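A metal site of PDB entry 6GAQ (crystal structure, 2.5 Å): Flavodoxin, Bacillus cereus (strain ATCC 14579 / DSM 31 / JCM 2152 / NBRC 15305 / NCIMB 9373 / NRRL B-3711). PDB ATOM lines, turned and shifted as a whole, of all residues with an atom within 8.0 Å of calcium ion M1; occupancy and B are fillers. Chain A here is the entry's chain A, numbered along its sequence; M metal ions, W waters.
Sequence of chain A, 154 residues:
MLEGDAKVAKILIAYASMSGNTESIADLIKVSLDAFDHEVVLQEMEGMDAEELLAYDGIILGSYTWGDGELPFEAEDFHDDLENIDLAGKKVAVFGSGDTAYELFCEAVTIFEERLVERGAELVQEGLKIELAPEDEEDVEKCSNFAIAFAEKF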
ATOM      1  N   ASN A  21      -5.334 -12.130   8.110  1.00  0.00           N
ATOM      2  CA  ASN A  21      -6.418 -11.277   7.619  1.00  0.00           C
ATOM      3  C   ASN A  21      -6.864 -11.697   6.229  1.00  0.00           C
ATOM      4  O   ASN A  21      -8.064 -11.868   5.971  1.00  0.00           O
ATOM      5  CB  ASN A  21      -5.979  -9.815   7.636  1.00  0.00           C
ATOM      6  CG  ASN A  21      -5.515  -9.357   8.998  1.00  0.00           C
ATOM      7  OD1 ASN A  21      -6.036  -9.799  10.025  1.00  0.00           O
ATOM      8  ND2 ASN A  21      -4.528  -8.467   9.015  1.00  0.00           N
ATOM      9  N   ILE A  25     -10.412 -13.598   4.763  1.00  0.00           N
ATOM     10  CA  ILE A  25     -11.173 -13.184   3.591  1.00  0.00           C
ATOM     11  C   ILE A  25     -11.358 -14.370   2.647  1.00  0.00           C
ATOM     12  O   ILE A  25     -12.435 -14.573   2.081  1.00  0.00           O
ATOM     13  CB  ILE A  25     -10.486 -12.007   2.889  1.00  0.00           C
ATOM     14  CG1 ILE A  25     -10.305 -10.833   3.854  1.00  0.00           C
ATOM     15  CG2 ILE A  25     -11.292 -11.568   1.681  1.00  0.00           C
ATOM     16  CD1 ILE A  25      -9.376  -9.763   3.340  1.00  0.00           C
ATOM     17  N   SER A  97      -6.059  -7.650   1.705  1.00  0.00           N
ATOM     18  CA  SER A  97      -6.221  -6.932   2.972  1.00  0.00           C
ATOM     19  C   SER A  97      -5.031  -6.015   3.170  1.00  0.00           C
ATOM     20  O   SER A  97      -3.877  -6.474   3.154  1.00  0.00           O
ATOM     21  CB  SER A  97      -6.355  -7.918   4.138  1.00  0.00           C
ATOM     22  OG  SER A  97      -6.387  -7.230   5.379  1.00  0.00           O
ATOM     23  N   GLY A  98      -5.294  -4.720   3.377  1.00  0.00           N
ATOM     24  CA  GLY A  98      -4.270  -3.732   3.593  1.00  0.00           C
ATOM     25  C   GLY A  98      -4.531  -2.921   4.851  1.00  0.00           C
ATOM     26  O   GLY A  98      -5.190  -3.369   5.784  1.00  0.00           O
ATOM     27  N   ILE A 130     -10.065  -4.958   1.570  1.00  0.00           N
ATOM     28  CA  ILE A 130     -10.463  -4.998   2.970  1.00  0.00           C
ATOM     29  C   ILE A 130      -9.334  -4.397   3.794  1.00  0.00           C
ATOM     30  O   ILE A 130      -8.159  -4.595   3.470  1.00  0.00           O
ATOM     31  CB  ILE A 130     -10.777  -6.438   3.416  1.00  0.00           C
ATOM     32  CG1 ILE A 130     -12.038  -6.968   2.702  1.00  0.00           C
ATOM     33  CG2 ILE A 130     -10.931  -6.542   4.933  1.00  0.00           C
ATOM     34  CD1 ILE A 130     -13.352  -6.447   3.288  1.00  0.00           C
ATOM     35  N   GLU A 131      -9.685  -3.659   4.852  1.00  0.00           N
ATOM     36  CA  GLU A 131      -8.671  -3.097   5.738  1.00  0.00           C
ATOM     37  C   GLU A 131      -8.502  -4.011   6.939  1.00  0.00           C
ATOM     38  O   GLU A 131      -9.452  -4.252   7.697  1.00  0.00           O
ATOM     39  CB  GLU A 131      -9.034  -1.678   6.163  1.00  0.00           C
ATOM     40  CG  GLU A 131      -8.277  -1.194   7.404  1.00  0.00           C
ATOM     41  CD  GLU A 131      -8.250   0.328   7.512  1.00  0.00           C
ATOM     42  OE1 GLU A 131      -7.239   0.878   8.015  1.00  0.00           O
ATOM     43  OE2 GLU A 131      -9.230   0.984   7.114  1.00  0.00           O
ATOM     44  N   LEU A 132      -7.282  -4.542   7.094  1.00  0.00           N
ATOM     45  CA  LEU A 132      -6.911  -5.407   8.221  1.00  0.00           C
ATOM     46  C   LEU A 132      -7.797  -6.654   8.155  1.00  0.00           C
ATOM     47  O   LEU A 132      -7.996  -7.179   7.045  1.00  0.00           O
ATOM     48  CB  LEU A 132      -7.007  -4.603   9.525  1.00  0.00           C
ATOM     49  CG  LEU A 132      -5.964  -3.493   9.700  1.00  0.00           C
ATOM     50  CD1 LEU A 132      -6.095  -2.849  11.073  1.00  0.00           C
ATOM     51  CD2 LEU A 132      -4.571  -4.050   9.484  1.00  0.00           C
ATOM     52  N   ALA A 133      -8.350  -7.139   9.280  1.00  0.00           N
ATOM     53  CA  ALA A 133      -9.190  -8.327   9.293  1.00  0.00           C
ATOM     54  C   ALA A 133     -10.645  -7.972   8.990  1.00  0.00           C
ATOM     55  O   ALA A 133     -11.103  -6.881   9.341  1.00  0.00           O
ATOM     56  CB  ALA A 133      -9.112  -9.007  10.655  1.00  0.00           C
ATOM     57  N   PRO A 134     -11.376  -8.869   8.328  1.00  0.00           N
ATOM     58  CA  PRO A 134     -12.814  -8.656   8.095  1.00  0.00           C
ATOM     59  C   PRO A 134     -13.647  -8.963   9.336  1.00  0.00           C
ATOM     60  O   PRO A 134     -14.465  -9.889   9.358  1.00  0.00           O
ATOM     61  CB  PRO A 134     -13.106  -9.604   6.939  1.00  0.00           C
ATOM     62  CG  PRO A 134     -12.166 -10.740   7.163  1.00  0.00           C
ATOM     63  CD  PRO A 134     -10.905 -10.136   7.729  1.00  0.00           C
ATOM     64  N   GLU A 135     -13.431  -8.178  10.392  1.00  0.00           N
ATOM     65  CA  GLU A 135     -13.937  -8.488  11.724  1.00  0.00           C
ATOM     66  C   GLU A 135     -15.108  -7.590  12.144  1.00  0.00           C
ATOM     67  O   GLU A 135     -15.312  -7.352  13.337  1.00  0.00           O
ATOM     68  CB  GLU A 135     -12.809  -8.394  12.751  1.00  0.00           C
ATOM     69  CG  GLU A 135     -12.200  -7.021  12.890  1.00  0.00           C
ATOM     70  CD  GLU A 135     -10.899  -7.027  13.679  1.00  0.00           C
ATOM     71  OE1 GLU A 135      -9.831  -6.808  13.072  1.00  0.00           O
ATOM     72  OE2 GLU A 135     -10.958  -7.257  14.901  1.00  0.00           O
ATOM     73  N   ASP A 136     -15.878  -7.074  11.184  1.00  0.00           N
ATOM     74  CA  ASP A 136     -17.065  -6.297  11.505  1.00  0.00           C
ATOM     75  C   ASP A 136     -18.113  -6.554  10.429  1.00  0.00           C
ATOM     76  O   ASP A 136     -17.862  -7.241   9.433  1.00  0.00           O
ATOM     77  CB  ASP A 136     -16.742  -4.811  11.660  1.00  0.00           C
ATOM     78  CG  ASP A 136     -16.484  -4.132  10.340  1.00  0.00           C
ATOM     79  OD1 ASP A 136     -15.633  -4.622   9.568  1.00  0.00           O
ATOM     80  OD2 ASP A 136     -17.127  -3.095  10.071  1.00  0.00           O
ATOM     81  N   GLU A 138     -19.809  -4.719   8.107  1.00  0.00           N
ATOM     82  CA  GLU A 138     -19.705  -4.262   6.732  1.00  0.00           C
ATOM     83  C   GLU A 138     -18.496  -4.820   6.003  1.00  0.00           C
ATOM     84  O   GLU A 138     -18.465  -4.789   4.774  1.00  0.00           O
ATOM     85  CB  GLU A 138     -19.701  -2.727   6.663  1.00  0.00           C
ATOM     86  CG  GLU A 138     -18.893  -2.035   7.736  1.00  0.00           C
ATOM     87  CD  GLU A 138     -19.230  -0.564   7.858  1.00  0.00           C
ATOM     88  OE1 GLU A 138     -18.407   0.206   8.394  1.00  0.00           O
ATOM     89  OE2 GLU A 138     -20.335  -0.173   7.407  1.00  0.00           O
ATOM     90  N   ASP A 139     -17.494  -5.341   6.727  1.00  0.00           N
ATOM     91  CA  ASP A 139     -16.427  -6.074   6.058  1.00  0.00           C
ATOM     92  C   ASP A 139     -16.923  -7.451   5.610  1.00  0.00           C
ATOM     93  O   ASP A 139     -16.605  -7.893   4.503  1.00  0.00           O
ATOM     94  CB  ASP A 139     -15.219  -6.228   6.979  1.00  0.00           C
ATOM     95  CG  ASP A 139     -14.175  -5.161   6.751  1.00  0.00           C
ATOM     96  OD1 ASP A 139     -13.025  -5.356   7.197  1.00  0.00           O
ATOM     97  OD2 ASP A 139     -14.495  -4.129   6.121  1.00  0.00           O
ATOM     98  N   VAL A 140     -17.688  -8.126   6.461  1.00  0.00           N
ATOM     99  CA  VAL A 140     -18.278  -9.409   6.082  1.00  0.00           C
ATOM    100  C   VAL A 140     -19.238  -9.222   4.911  1.00  0.00           C
ATOM    101  O   VAL A 140     -19.307 -10.072   4.007  1.00  0.00           O
ATOM    102  CB  VAL A 140     -18.984 -10.041   7.295  1.00  0.00           C
ATOM    103  CG1 VAL A 140     -19.674 -11.337   6.900  1.00  0.00           C
ATOM    104  CG2 VAL A 140     -17.988 -10.289   8.424  1.00  0.00           C
ATOM    105  N   LYS A 142     -18.951  -6.832   2.681  1.00  0.00           N
ATOM    106  CA  LYS A 142     -18.109  -6.554   1.525  1.00  0.00           C
ATOM    107  C   LYS A 142     -17.660  -7.838   0.855  1.00  0.00           C
ATOM    108  O   LYS A 142     -17.720  -7.977  -0.378  1.00  0.00           O
ATOM    109  CB  LYS A 142     -16.906  -5.706   1.928  1.00  0.00           C
ATOM    110  CG  LYS A 142     -17.161  -4.207   1.938  1.00  0.00           C
ATOM    111  CD  LYS A 142     -16.066  -3.459   2.692  1.00  0.00           C
ATOM    112  CE  LYS A 142     -14.818  -3.294   1.840  1.00  0.00           C
ATOM    113  NZ  LYS A 142     -13.775  -2.501   2.544  1.00  0.00           N
HETATM  114 CA    CA M   1     -11.595  -4.534   8.898  1.00  0.00          CA
HETATM  115 CA    CA M   2     -16.273  -0.761   9.174  1.00  0.00          CA
HETATM  116  O   HOH W   1     -10.277  -4.077  10.928  1.00  0.00           O
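The side-chain carboxylate of Asp 136 sits close to the backbone NH of Asp 139.
OD2 of Asp 139 lies within salt-bridge range of NZ of Lys 142 (3.995 Å).
The side-chain carboxylate (OD1) of Asp 139 is bound to calcium ion M1 (2.4 Å).
O of Ala 133 binds calcium ion M1 (2.4 Å).
Calcium ion M1 is bound by water W1 (2.5 Å).
Calcium ion M1 is bound by O of Glu 131 (2.5 Å).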
